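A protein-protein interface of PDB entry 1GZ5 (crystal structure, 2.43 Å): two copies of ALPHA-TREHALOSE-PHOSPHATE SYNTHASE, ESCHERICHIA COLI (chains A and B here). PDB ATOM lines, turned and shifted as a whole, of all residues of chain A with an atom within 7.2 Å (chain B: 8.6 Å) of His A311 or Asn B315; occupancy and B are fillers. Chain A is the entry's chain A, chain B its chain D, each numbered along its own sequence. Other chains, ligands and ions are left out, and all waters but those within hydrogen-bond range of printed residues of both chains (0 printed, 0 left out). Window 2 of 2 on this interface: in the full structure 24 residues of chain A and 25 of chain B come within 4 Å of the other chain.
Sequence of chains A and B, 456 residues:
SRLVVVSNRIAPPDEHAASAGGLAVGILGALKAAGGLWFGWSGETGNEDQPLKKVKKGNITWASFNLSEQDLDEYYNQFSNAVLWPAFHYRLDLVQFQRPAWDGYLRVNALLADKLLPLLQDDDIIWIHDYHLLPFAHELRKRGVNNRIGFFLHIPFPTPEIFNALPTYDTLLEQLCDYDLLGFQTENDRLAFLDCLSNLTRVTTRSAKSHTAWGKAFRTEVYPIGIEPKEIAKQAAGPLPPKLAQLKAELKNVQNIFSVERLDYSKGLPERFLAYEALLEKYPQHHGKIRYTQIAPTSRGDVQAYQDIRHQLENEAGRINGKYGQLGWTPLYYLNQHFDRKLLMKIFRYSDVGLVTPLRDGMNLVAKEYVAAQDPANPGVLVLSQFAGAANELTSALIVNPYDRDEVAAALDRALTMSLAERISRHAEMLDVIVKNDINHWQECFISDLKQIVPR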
ATOM      1  N   LEU A 263       1.431  -4.791 -27.214  1.00  0.00           N
ATOM      2  CA  LEU A 263       0.546  -3.806 -27.721  1.00  0.00           C
ATOM      3  C   LEU A 263       0.755  -3.650 -29.201  1.00  0.00           C
ATOM      4  O   LEU A 263       1.496  -2.753 -29.649  1.00  0.00           O
ATOM      5  CB  LEU A 263       0.775  -2.486 -27.010  1.00  0.00           C
ATOM      6  CG  LEU A 263      -0.484  -1.611 -26.786  1.00  0.00           C
ATOM      7  CD1 LEU A 263      -0.124  -0.425 -25.896  1.00  0.00           C
ATOM      8  CD2 LEU A 263      -1.045  -1.108 -28.091  1.00  0.00           C
ATOM      9  N   GLN A 304       5.443   4.274 -36.251  1.00  0.00           N
ATOM     10  CA  GLN A 304       4.294   5.148 -36.128  1.00  0.00           C
ATOM     11  C   GLN A 304       3.017   4.400 -35.868  1.00  0.00           C
ATOM     12  O   GLN A 304       2.276   4.754 -34.961  1.00  0.00           O
ATOM     13  CB  GLN A 304       4.151   6.053 -37.360  1.00  0.00           C
ATOM     14  CG  GLN A 304       2.991   7.069 -37.235  1.00  0.00           C
ATOM     15  CD  GLN A 304       3.274   8.095 -36.167  1.00  0.00           C
ATOM     16  OE1 GLN A 304       2.432   8.339 -35.292  1.00  0.00           O
ATOM     17  NE2 GLN A 304       4.461   8.661 -36.187  1.00  0.00           N
ATOM     18  N   TYR A 306       2.467   1.745 -34.358  1.00  0.00           N
ATOM     19  CA  TYR A 306       2.401   1.248 -32.969  1.00  0.00           C
ATOM     20  C   TYR A 306       2.073   2.324 -31.951  1.00  0.00           C
ATOM     21  O   TYR A 306       1.279   2.085 -31.053  1.00  0.00           O
ATOM     22  CB  TYR A 306       3.665   0.487 -32.578  1.00  0.00           C
ATOM     23  CG  TYR A 306       3.698  -0.886 -33.202  1.00  0.00           C
ATOM     24  CD1 TYR A 306       4.175  -1.066 -34.502  1.00  0.00           C
ATOM     25  CD2 TYR A 306       3.247  -2.003 -32.494  1.00  0.00           C
ATOM     26  CE1 TYR A 306       4.188  -2.345 -35.105  1.00  0.00           C
ATOM     27  CE2 TYR A 306       3.264  -3.265 -33.067  1.00  0.00           C
ATOM     28  CZ  TYR A 306       3.734  -3.438 -34.368  1.00  0.00           C
ATOM     29  OH  TYR A 306       3.786  -4.686 -34.919  1.00  0.00           O
ATOM     30  N   GLN A 307       2.679   3.493 -32.099  1.00  0.00           N
ATOM     31  CA  GLN A 307       2.271   4.703 -31.386  1.00  0.00           C
ATOM     32  C   GLN A 307       0.785   4.984 -31.569  1.00  0.00           C
ATOM     33  O   GLN A 307       0.088   5.223 -30.583  1.00  0.00           O
ATOM     34  CB  GLN A 307       3.093   5.918 -31.833  1.00  0.00           C
ATOM     35  CG  GLN A 307       4.573   5.798 -31.527  1.00  0.00           C
ATOM     36  CD  GLN A 307       5.456   6.811 -32.304  1.00  0.00           C
ATOM     37  OE1 GLN A 307       5.036   7.951 -32.620  1.00  0.00           O
ATOM     38  NE2 GLN A 307       6.689   6.396 -32.607  1.00  0.00           N
ATOM     39  N   ASP A 308       0.278   4.942 -32.806  1.00  0.00           N
ATOM     40  CA  ASP A 308      -1.156   5.257 -33.019  1.00  0.00           C
ATOM     41  C   ASP A 308      -2.075   4.286 -32.236  1.00  0.00           C
ATOM     42  O   ASP A 308      -3.005   4.679 -31.566  1.00  0.00           O
ATOM     43  CB  ASP A 308      -1.510   5.185 -34.502  1.00  0.00           C
ATOM     44  CG  ASP A 308      -0.817   6.225 -35.336  1.00  0.00           C
ATOM     45  OD1 ASP A 308      -0.229   7.220 -34.830  1.00  0.00           O
ATOM     46  OD2 ASP A 308      -0.791   6.137 -36.583  1.00  0.00           O
ATOM     47  N   ILE A 309      -1.793   3.000 -32.279  1.00  0.00           N
ATOM     48  CA  ILE A 309      -2.698   2.056 -31.657  1.00  0.00           C
ATOM     49  C   ILE A 309      -2.644   2.202 -30.148  1.00  0.00           C
ATOM     50  O   ILE A 309      -3.667   2.108 -29.456  1.00  0.00           O
ATOM     51  CB  ILE A 309      -2.370   0.594 -32.150  1.00  0.00           C
ATOM     52  CG1 ILE A 309      -3.429  -0.356 -31.597  1.00  0.00           C
ATOM     53  CG2 ILE A 309      -1.017   0.076 -31.716  1.00  0.00           C
ATOM     54  CD1 ILE A 309      -4.621  -0.288 -32.725  1.00  0.00           C
ATOM     55  N   ARG A 310      -1.449   2.524 -29.636  1.00  0.00           N
ATOM     56  CA  ARG A 310      -1.312   2.796 -28.233  1.00  0.00           C
ATOM     57  C   ARG A 310      -2.116   4.014 -27.773  1.00  0.00           C
ATOM     58  O   ARG A 310      -2.779   3.979 -26.768  1.00  0.00           O
ATOM     59  CB  ARG A 310       0.145   3.025 -27.952  1.00  0.00           C
ATOM     60  CG  ARG A 310       0.421   3.269 -26.515  1.00  0.00           C
ATOM     61  CD  ARG A 310       1.922   2.998 -26.335  1.00  0.00           C
ATOM     62  NE  ARG A 310       2.358   3.625 -25.137  1.00  0.00           N
ATOM     63  CZ  ARG A 310       2.938   4.793 -25.109  1.00  0.00           C
ATOM     64  NH1 ARG A 310       3.190   5.382 -26.310  1.00  0.00           N
ATOM     65  NH2 ARG A 310       3.256   5.346 -23.883  1.00  0.00           N
ATOM     66  N   HIS A 311      -2.051   5.107 -28.519  1.00  0.00           N
ATOM     67  CA  HIS A 311      -2.822   6.286 -28.146  1.00  0.00           C
ATOM     68  C   HIS A 311      -4.305   5.985 -28.205  1.00  0.00           C
ATOM     69  O   HIS A 311      -5.058   6.409 -27.326  1.00  0.00           O
ATOM     70  CB  HIS A 311      -2.492   7.468 -29.025  1.00  0.00           C
ATOM     71  CG  HIS A 311      -1.090   7.932 -28.874  1.00  0.00           C
ATOM     72  ND1 HIS A 311      -0.477   8.052 -27.633  1.00  0.00           N
ATOM     73  CD2 HIS A 311      -0.155   8.300 -29.796  1.00  0.00           C
ATOM     74  CE1 HIS A 311       0.766   8.495 -27.801  1.00  0.00           C
ATOM     75  NE2 HIS A 311       0.982   8.666 -29.099  1.00  0.00           N
ATOM     76  N   GLN A 312      -4.713   5.213 -29.204  1.00  0.00           N
ATOM     77  CA  GLN A 312      -6.105   4.863 -29.328  1.00  0.00           C
ATOM     78  C   GLN A 312      -6.548   4.001 -28.091  1.00  0.00           C
ATOM     79  O   GLN A 312      -7.603   4.210 -27.465  1.00  0.00           O
ATOM     80  CB  GLN A 312      -6.296   4.139 -30.683  1.00  0.00           C
ATOM     81  CG  GLN A 312      -7.675   3.550 -30.871  1.00  0.00           C
ATOM     82  CD  GLN A 312      -7.930   2.930 -32.328  1.00  0.00           C
ATOM     83  OE1 GLN A 312      -9.027   2.359 -32.588  1.00  0.00           O
ATOM     84  NE2 GLN A 312      -6.938   3.050 -33.240  1.00  0.00           N
ATOM     85  N   LEU A 313      -5.702   3.063 -27.710  1.00  0.00           N
ATOM     86  CA  LEU A 313      -6.022   2.239 -26.567  1.00  0.00           C
ATOM     87  C   LEU A 313      -6.114   3.059 -25.280  1.00  0.00           C
ATOM     88  O   LEU A 313      -7.022   2.849 -24.484  1.00  0.00           O
ATOM     89  CB  LEU A 313      -5.007   1.102 -26.483  1.00  0.00           C
ATOM     90  CG  LEU A 313      -5.564  -0.194 -25.933  1.00  0.00           C
ATOM     91  CD1 LEU A 313      -6.800  -0.641 -26.748  1.00  0.00           C
ATOM     92  CD2 LEU A 313      -4.464  -1.325 -25.788  1.00  0.00           C
ATOM     93  N   GLU A 314      -5.230   4.033 -25.078  1.00  0.00           N
ATOM     94  CA  GLU A 314      -5.308   4.881 -23.870  1.00  0.00           C
ATOM     95  C   GLU A 314      -6.632   5.646 -23.855  1.00  0.00           C
ATOM     96  O   GLU A 314      -7.256   5.861 -22.772  1.00  0.00           O
ATOM     97  CB  GLU A 314      -4.188   5.913 -23.832  1.00  0.00           C
ATOM     98  CG  GLU A 314      -2.793   5.375 -23.562  1.00  0.00           C
ATOM     99  CD  GLU A 314      -1.680   6.307 -24.008  1.00  0.00           C
ATOM    100  OE1 GLU A 314      -1.911   7.371 -24.701  1.00  0.00           O
ATOM    101  OE2 GLU A 314      -0.518   5.986 -23.645  1.00  0.00           O
ATOM    102  N   ASN A 315      -7.104   6.031 -25.039  1.00  0.00           N
ATOM    103  CA  ASN A 315      -8.325   6.814 -25.097  1.00  0.00           C
ATOM    104  C   ASN A 315      -9.519   5.968 -24.683  1.00  0.00           C
ATOM    105  O   ASN A 315     -10.356   6.405 -23.904  1.00  0.00           O
ATOM    106  CB  ASN A 315      -8.553   7.437 -26.487  1.00  0.00           C
ATOM    107  CG  ASN A 315      -9.837   8.316 -26.521  1.00  0.00           C
ATOM    108  OD1 ASN A 315     -10.994   7.814 -26.802  1.00  0.00           O
ATOM    109  ND2 ASN A 315      -9.666   9.642 -26.166  1.00  0.00           N
ATOM    110  N   GLU A 316      -9.586   4.744 -25.197  1.00  0.00           N
ATOM    111  CA  GLU A 316     -10.674   3.856 -24.897  1.00  0.00           C
ATOM    112  C   GLU A 316     -10.678   3.440 -23.427  1.00  0.00           C
ATOM    113  O   GLU A 316     -11.749   3.340 -22.841  1.00  0.00           O
ATOM    114  CB  GLU A 316     -10.644   2.634 -25.810  1.00  0.00           C
ATOM    115  CG  GLU A 316     -10.929   3.050 -27.242  1.00  0.00           C
ATOM    116  CD  GLU A 316     -12.431   3.358 -27.413  1.00  0.00           C
ATOM    117  OE1 GLU A 316     -13.169   2.410 -27.618  1.00  0.00           O
ATOM    118  OE2 GLU A 316     -12.907   4.490 -27.256  1.00  0.00           O
ATOM    119  N   ALA A 317      -9.518   3.217 -22.817  1.00  0.00           N
ATOM    120  CA  ALA A 317      -9.519   2.911 -21.382  1.00  0.00           C
ATOM    121  C   ALA A 317     -10.122   4.077 -20.557  1.00  0.00           C
ATOM    122  O   ALA A 317     -10.945   3.879 -19.704  1.00  0.00           O
ATOM    123  CB  ALA A 317      -8.102   2.562 -20.891  1.00  0.00           C
ATOM    124  N   GLY A 318      -9.658   5.296 -20.812  1.00  0.00           N
ATOM    125  CA  GLY A 318     -10.172   6.467 -20.152  1.00  0.00           C
ATOM    126  C   GLY A 318     -11.647   6.586 -20.430  1.00  0.00           C
ATOM    127  O   GLY A 318     -12.440   6.855 -19.512  1.00  0.00           O
ATOM    128  N   ARG A 319     -12.048   6.370 -21.680  1.00  0.00           N
ATOM    129  CA  ARG A 319     -13.475   6.557 -22.012  1.00  0.00           C
ATOM    130  C   ARG A 319     -14.374   5.541 -21.305  1.00  0.00           C
ATOM    131  O   ARG A 319     -15.386   5.908 -20.745  1.00  0.00           O
ATOM    132  CB  ARG A 319     -13.732   6.569 -23.513  1.00  0.00           C
ATOM    133  CG  ARG A 319     -15.172   6.874 -23.932  1.00  0.00           C
ATOM    134  CD  ARG A 319     -15.387   6.688 -25.451  1.00  0.00           C
ATOM    135  NE  ARG A 319     -15.186   5.314 -25.889  1.00  0.00           N
ATOM    136  CZ  ARG A 319     -16.108   4.330 -25.788  1.00  0.00           C
ATOM    137  NH1 ARG A 319     -17.286   4.561 -25.255  1.00  0.00           N
ATOM    138  NH2 ARG A 319     -15.848   3.107 -26.230  1.00  0.00           N
ATOM    139  N   TYR A 334      -6.209  -1.366 -17.452  1.00  0.00           N
ATOM    140  CA  TYR A 334      -5.311  -1.406 -18.551  1.00  0.00           C
ATOM    141  C   TYR A 334      -3.921  -1.134 -18.061  1.00  0.00           C
ATOM    142  O   TYR A 334      -3.673  -0.135 -17.426  1.00  0.00           O
ATOM    143  CB  TYR A 334      -5.756  -0.374 -19.565  1.00  0.00           C
ATOM    144  CG  TYR A 334      -4.709   0.023 -20.589  1.00  0.00           C
ATOM    145  CD1 TYR A 334      -4.160  -0.900 -21.480  1.00  0.00           C
ATOM    146  CD2 TYR A 334      -4.267   1.328 -20.632  1.00  0.00           C
ATOM    147  CE1 TYR A 334      -3.168  -0.495 -22.405  1.00  0.00           C
ATOM    148  CE2 TYR A 334      -3.303   1.734 -21.527  1.00  0.00           C
ATOM    149  CZ  TYR A 334      -2.748   0.808 -22.415  1.00  0.00           C
ATOM    150  OH  TYR A 334      -1.786   1.259 -23.309  1.00  0.00           O
ATOM    151  N   PHE B 273      -3.992  16.281 -13.851  1.00  0.00           N
ATOM    152  CA  PHE B 273      -3.581  14.888 -14.042  1.00  0.00           C
ATOM    153  C   PHE B 273      -2.044  14.821 -14.053  1.00  0.00           C
ATOM    154  O   PHE B 273      -1.420  13.932 -13.477  1.00  0.00           O
ATOM    155  CB  PHE B 273      -4.195  14.315 -15.318  1.00  0.00           C
ATOM    156  CG  PHE B 273      -5.649  13.889 -15.182  1.00  0.00           C
ATOM    157  CD1 PHE B 273      -6.468  14.408 -14.175  1.00  0.00           C
ATOM    158  CD2 PHE B 273      -6.206  12.980 -16.082  1.00  0.00           C
ATOM    159  CE1 PHE B 273      -7.836  14.030 -14.068  1.00  0.00           C
ATOM    160  CE2 PHE B 273      -7.539  12.578 -15.969  1.00  0.00           C
ATOM    161  CZ  PHE B 273      -8.358  13.118 -14.937  1.00  0.00           C
ATOM    162  N   ASP B 308     -12.708  18.649 -27.423  1.00  0.00           N
ATOM    163  CA  ASP B 308     -11.251  18.461 -27.400  1.00  0.00           C
ATOM    164  C   ASP B 308     -10.722  18.159 -25.996  1.00  0.00           C
ATOM    165  O   ASP B 308      -9.957  17.204 -25.816  1.00  0.00           O
ATOM    166  CB  ASP B 308     -10.491  19.653 -28.008  1.00  0.00           C
ATOM    167  CG  ASP B 308     -10.808  19.864 -29.483  1.00  0.00           C
ATOM    168  OD1 ASP B 308     -11.319  18.932 -30.198  1.00  0.00           O
ATOM    169  OD2 ASP B 308     -10.609  20.966 -30.033  1.00  0.00           O
ATOM    170  N   ILE B 309     -11.161  18.928 -25.007  1.00  0.00           N
ATOM    171  CA  ILE B 309     -10.579  18.800 -23.678  1.00  0.00           C
ATOM    172  C   ILE B 309     -10.971  17.457 -23.070  1.00  0.00           C
ATOM    173  O   ILE B 309     -10.203  16.799 -22.377  1.00  0.00           O
ATOM    174  CB  ILE B 309     -10.934  20.035 -22.760  1.00  0.00           C
ATOM    175  CG1 ILE B 309     -10.119  19.987 -21.481  1.00  0.00           C
ATOM    176  CG2 ILE B 309     -12.436  20.141 -22.436  1.00  0.00           C
ATOM    177  CD1 ILE B 309      -8.745  20.662 -21.680  1.00  0.00           C
ATOM    178  N   ARG B 310     -12.166  17.033 -23.395  1.00  0.00           N
ATOM    179  CA  ARG B 310     -12.651  15.755 -22.935  1.00  0.00           C
ATOM    180  C   ARG B 310     -11.859  14.585 -23.499  1.00  0.00           C
ATOM    181  O   ARG B 310     -11.520  13.638 -22.760  1.00  0.00           O
ATOM    182  CB  ARG B 310     -14.081  15.608 -23.381  1.00  0.00           C
ATOM    183  CG  ARG B 310     -14.718  14.374 -22.944  1.00  0.00           C
ATOM    184  CD  ARG B 310     -16.207  14.575 -22.969  1.00  0.00           C
ATOM    185  NE  ARG B 310     -16.816  13.285 -22.994  1.00  0.00           N
ATOM    186  CZ  ARG B 310     -17.236  12.719 -24.091  1.00  0.00           C
ATOM    187  NH1 ARG B 310     -17.115  13.381 -25.279  1.00  0.00           N
ATOM    188  NH2 ARG B 310     -17.726  11.468 -23.988  1.00  0.00           N
ATOM    189  N   HIS B 311     -11.584  14.615 -24.798  1.00  0.00           N
ATOM    190  CA  HIS B 311     -10.754  13.577 -25.411  1.00  0.00           C
ATOM    191  C   HIS B 311      -9.353  13.557 -24.807  1.00  0.00           C
ATOM    192  O   HIS B 311      -8.792  12.491 -24.563  1.00  0.00           O
ATOM    193  CB  HIS B 311     -10.680  13.744 -26.912  1.00  0.00           C
ATOM    194  CG  HIS B 311     -11.995  13.554 -27.597  1.00  0.00           C
ATOM    195  ND1 HIS B 311     -12.897  12.556 -27.229  1.00  0.00           N
ATOM    196  CD2 HIS B 311     -12.579  14.228 -28.627  1.00  0.00           C
ATOM    197  CE1 HIS B 311     -13.964  12.620 -28.019  1.00  0.00           C
ATOM    198  NE2 HIS B 311     -13.796  13.620 -28.878  1.00  0.00           N
ATOM    199  N   GLN B 312      -8.817  14.741 -24.528  1.00  0.00           N
ATOM    200  CA  GLN B 312      -7.498  14.846 -23.984  1.00  0.00           C
ATOM    201  C   GLN B 312      -7.528  14.256 -22.554  1.00  0.00           C
ATOM    202  O   GLN B 312      -6.651  13.519 -22.152  1.00  0.00           O
ATOM    203  CB  GLN B 312      -7.062  16.309 -24.025  1.00  0.00           C
ATOM    204  CG  GLN B 312      -5.765  16.592 -23.274  1.00  0.00           C
ATOM    205  CD  GLN B 312      -5.243  18.092 -23.387  1.00  0.00           C
ATOM    206  OE1 GLN B 312      -4.161  18.405 -22.835  1.00  0.00           O
ATOM    207  NE2 GLN B 312      -5.988  18.980 -24.114  1.00  0.00           N
ATOM    208  N   LEU B 313      -8.566  14.526 -21.812  1.00  0.00           N
ATOM    209  CA  LEU B 313      -8.649  13.987 -20.452  1.00  0.00           C
ATOM    210  C   LEU B 313      -8.797  12.447 -20.455  1.00  0.00           C
ATOM    211  O   LEU B 313      -8.149  11.766 -19.660  1.00  0.00           O
ATOM    212  CB  LEU B 313      -9.790  14.677 -19.686  1.00  0.00           C
ATOM    213  CG  LEU B 313      -9.535  14.871 -18.221  1.00  0.00           C
ATOM    214  CD1 LEU B 313      -8.279  15.637 -18.011  1.00  0.00           C
ATOM    215  CD2 LEU B 313     -10.778  15.535 -17.513  1.00  0.00           C
ATOM    216  N   GLU B 314      -9.602  11.894 -21.370  1.00  0.00           N
ATOM    217  CA  GLU B 314      -9.691  10.438 -21.506  1.00  0.00           C
ATOM    218  C   GLU B 314      -8.346   9.833 -21.813  1.00  0.00           C
ATOM    219  O   GLU B 314      -8.011   8.783 -21.289  1.00  0.00           O
ATOM    220  CB  GLU B 314     -10.613  10.009 -22.618  1.00  0.00           C
ATOM    221  CG  GLU B 314     -12.095  10.212 -22.361  1.00  0.00           C
ATOM    222  CD  GLU B 314     -12.925  10.367 -23.651  1.00  0.00           C
ATOM    223  OE1 GLU B 314     -12.368  10.423 -24.808  1.00  0.00           O
ATOM    224  OE2 GLU B 314     -14.170  10.382 -23.507  1.00  0.00           O
ATOM    225  N   ASN B 315      -7.543  10.504 -22.633  1.00  0.00           N
ATOM    226  CA  ASN B 315      -6.209   9.972 -22.963  1.00  0.00           C
ATOM    227  C   ASN B 315      -5.285   9.921 -21.740  1.00  0.00           C
ATOM    228  O   ASN B 315      -4.639   8.883 -21.483  1.00  0.00           O
ATOM    229  CB  ASN B 315      -5.547  10.722 -24.100  1.00  0.00           C
ATOM    230  CG  ASN B 315      -4.201  10.084 -24.518  1.00  0.00           C
ATOM    231  OD1 ASN B 315      -3.094  10.466 -23.972  1.00  0.00           O
ATOM    232  ND2 ASN B 315      -4.252   9.114 -25.506  1.00  0.00           N
ATOM    233  N   GLU B 316      -5.277  11.005 -20.979  1.00  0.00           N
ATOM    234  CA  GLU B 316      -4.459  11.069 -19.835  1.00  0.00           C
ATOM    235  C   GLU B 316      -4.855  10.070 -18.734  1.00  0.00           C
ATOM    236  O   GLU B 316      -3.977   9.494 -18.127  1.00  0.00           O
ATOM    237  CB  GLU B 316      -4.414  12.488 -19.316  1.00  0.00           C
ATOM    238  CG  GLU B 316      -3.675  13.400 -20.268  1.00  0.00           C
ATOM    239  CD  GLU B 316      -2.157  13.179 -20.198  1.00  0.00           C
ATOM    240  OE1 GLU B 316      -1.531  13.858 -19.390  1.00  0.00           O
ATOM    241  OE2 GLU B 316      -1.613  12.303 -20.905  1.00  0.00           O
ATOM    242  N   ALA B 317      -6.142   9.850 -18.501  1.00  0.00           N
ATOM    243  CA  ALA B 317      -6.564   8.840 -17.552  1.00  0.00           C
ATOM    244  C   ALA B 317      -6.042   7.449 -17.932  1.00  0.00           C
ATOM    245  O   ALA B 317      -5.475   6.757 -17.089  1.00  0.00           O
ATOM    246  CB  ALA B 317      -8.090   8.826 -17.420  1.00  0.00           C
ATOM    247  N   GLY B 318      -6.249   7.050 -19.190  1.00  0.00           N
ATOM    248  CA  GLY B 318      -5.777   5.787 -19.699  1.00  0.00           C
ATOM    249  C   GLY B 318      -4.258   5.721 -19.611  1.00  0.00           C
ATOM    250  O   GLY B 318      -3.721   4.703 -19.197  1.00  0.00           O
ATOM    251  N   ARG B 319      -3.564   6.809 -19.918  1.00  0.00           N
ATOM    252  CA  ARG B 319      -2.105   6.782 -19.893  1.00  0.00           C
ATOM    253  C   ARG B 319      -1.537   6.633 -18.470  1.00  0.00           C
ATOM    254  O   ARG B 319      -0.658   5.814 -18.211  1.00  0.00           O
ATOM    255  CB  ARG B 319      -1.502   8.006 -20.617  1.00  0.00           C
ATOM    256  CG  ARG B 319       0.031   8.000 -20.716  1.00  0.00           C
ATOM    257  CD  ARG B 319       0.622   9.278 -21.253  1.00  0.00           C
ATOM    258  NE  ARG B 319       0.374  10.424 -20.390  1.00  0.00           N
ATOM    259  CZ  ARG B 319       1.066  10.740 -19.285  1.00  0.00           C
ATOM    260  NH1 ARG B 319       2.076  10.001 -18.872  1.00  0.00           N
ATOM    261  NH2 ARG B 319       0.736  11.819 -18.575  1.00  0.00           N
ATOM    262  N   ILE B 320      -2.088   7.415 -17.548  1.00  0.00           N
ATOM    263  CA  ILE B 320      -1.553   7.454 -16.196  1.00  0.00           C
ATOM    264  C   ILE B 320      -1.805   6.130 -15.456  1.00  0.00           C
ATOM    265  O   ILE B 320      -0.876   5.553 -14.873  1.00  0.00           O
ATOM    266  CB  ILE B 320      -2.093   8.655 -15.458  1.00  0.00           C
ATOM    267  CG1 ILE B 320      -1.436   9.906 -16.020  1.00  0.00           C
ATOM    268  CG2 ILE B 320      -1.778   8.535 -13.922  1.00  0.00           C
ATOM    269  CD1 ILE B 320      -2.145  11.171 -15.553  1.00  0.00           C
ATOM    270  N   ASN B 321      -3.037   5.624 -15.559  1.00  0.00           N
ATOM    271  CA  ASN B 321      -3.337   4.328 -15.029  1.00  0.00           C
ATOM    272  C   ASN B 321      -2.538   3.248 -15.709  1.00  0.00           C
ATOM    273  O   ASN B 321      -2.094   2.326 -15.042  1.00  0.00           O
ATOM    274  CB  ASN B 321      -4.834   4.055 -15.053  1.00  0.00           C
ATOM    275  CG  ASN B 321      -5.574   4.846 -13.988  1.00  0.00           C
ATOM    276  OD1 ASN B 321      -5.042   5.098 -12.900  1.00  0.00           O
ATOM    277  ND2 ASN B 321      -6.753   5.252 -14.285  1.00  0.00           N
ATOM    278  N   GLY B 322      -2.277   3.392 -17.004  1.00  0.00           N
ATOM    279  CA  GLY B 322      -1.570   2.352 -17.711  1.00  0.00           C
ATOM    280  C   GLY B 322      -0.128   2.247 -17.277  1.00  0.00           C
ATOM    281  O   GLY B 322       0.484   1.207 -17.360  1.00  0.00           O
ATOM    282  N   LEU B 332      -5.940   6.431 -10.303  1.00  0.00           N
ATOM    283  CA  LEU B 332      -6.758   7.547 -10.725  1.00  0.00           C
ATOM    284  C   LEU B 332      -8.126   7.079 -11.187  1.00  0.00           C
ATOM    285  O   LEU B 332      -8.196   6.290 -12.077  1.00  0.00           O
ATOM    286  CB  LEU B 332      -6.086   8.244 -11.901  1.00  0.00           C
ATOM    287  CG  LEU B 332      -6.525   9.663 -12.200  1.00  0.00           C
ATOM    288  CD1 LEU B 332      -5.555  10.328 -13.163  1.00  0.00           C
ATOM    289  CD2 LEU B 332      -7.844   9.651 -12.785  1.00  0.00           C
ATOM    290  N   TYR B 334     -11.292   8.379 -12.885  1.00  0.00           N
ATOM    291  CA  TYR B 334     -11.887   9.466 -13.637  1.00  0.00           C
ATOM    292  C   TYR B 334     -13.321   9.088 -14.006  1.00  0.00           C
ATOM    293  O   TYR B 334     -13.570   8.058 -14.565  1.00  0.00           O
ATOM    294  CB  TYR B 334     -11.033   9.751 -14.844  1.00  0.00           C
ATOM    295  CG  TYR B 334     -11.732  10.489 -15.959  1.00  0.00           C
ATOM    296  CD1 TYR B 334     -12.156  11.812 -15.799  1.00  0.00           C
ATOM    297  CD2 TYR B 334     -11.965   9.866 -17.168  1.00  0.00           C
ATOM    298  CE1 TYR B 334     -12.807  12.491 -16.836  1.00  0.00           C
ATOM    299  CE2 TYR B 334     -12.618  10.533 -18.197  1.00  0.00           C
ATOM    300  CZ  TYR B 334     -13.038  11.851 -18.008  1.00  0.00           C
ATOM    301  OH  TYR B 334     -13.692  12.483 -19.048  1.00  0.00           O
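O of His A311 is in hydrogen-bond range of ND2 of Asn B315. The side-chain carboxylate of Glu A314 is in hydrogen-bond range of the side-chain amide nitrogen of Asn B315 (3.0 Å). ND2 of Asn A315 is in hydrogen-bond range of O of His B311, 3.4 Å away. ND2 of Asn A315 sits at hydrogen-bond distance from OE1 of Glu B314 (3.1 Å). O of Glu A314 sits close to O of Glu B314 (3.4 Å).
NH2 of Arg A310 is in salt-bridge range of OE2 of Glu A314 (3.8 Å). A ring nitrogen (ND1) of His A311 sits at hydrogen-bond distance from the side-chain carboxylate (OE1) of Glu A314 (3.3 Å). The side-chain carboxylate (OE2) of Glu A316 is in salt-bridge range of the guanidinium group (NE) of Arg A319, at 2.8 Å. The side-chain carboxylate (OE1) of Glu B314 is in hydrogen-bond range of a ring nitrogen (ND1) of His B311, 3.3 Å away.
Among the printed residues, pairs that only touch across the chains: Glu A314 with Gly B318 (3.4 Å), Glu A314 with Arg B319 (3.6 Å), Gly A318 with Glu B314 (3.4 Å), Gly A318 with Tyr B334 (3.8 Å), Arg A319 with Glu B314 (3.7 Å), Tyr A334 with Gly B318 (3.7 Å), Tyr A334 with Asn B321 (3.8 Å) and Tyr A334 with Gly B322 (3.3 Å).
Arg A310 touches none of the printed residues of chain B. Of chain B, only Asn B315 comes within 4 Å of His A311. Glu A314 touches just these residues of chain B: Glu B314, Asn B315, Gly B318 and Arg B319. Ala A317 touches none of the printed residues of chain B. Of chain A, only His A311 (3.4 Å) and Glu A314 (3.0 Å) come within 4 Å of Asn B315. Of the printed residues of chain A, Gly B318 touches Glu A314 (3.4 Å) and Tyr A334 (3.7 Å). Of the printed residues of chain A, Tyr B334 touches Gly A318. The nearest residue of chain B that does not touch His A311 is Arg B319 (6.6 Å). The nearest printed residue of chain B that does not touch Gly A318 is Gly B318 (4.1 Å).
Hydrophobic or aromatic side chains of chain B within 4 Å of the printed part of chain A: Tyr B334. Printed residues of chain A that touch a printed residue of chain B: His A311, Glu A314, Asn A315, Gly A318, Arg A319 and Tyr A334. Hydrophobic or aromatic side chains of chain A that line the printed part of chain B: Tyr A334. Among the printed residues, no Asp or Glu carboxylate lies within 4 Å of a Lys or Arg side-chain nitrogen of the other chain.
Glu A314 touches its own counterpart, Glu B314. Glu A314 touches Asn B315, and with the chains exchanged Asn A315 touches Glu B314. Glu A314 touches Arg B319, and with the chains exchanged Arg A319 touches Glu B314. Positions printed for both chains: 308, 309, 310, 311, 312, 313, 314, 315, 316, 317, 318, 319 and 334. Of the 13 pairs that touch across the chains among the printed residues, 11 have their exchanged pair printed and touching as well.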
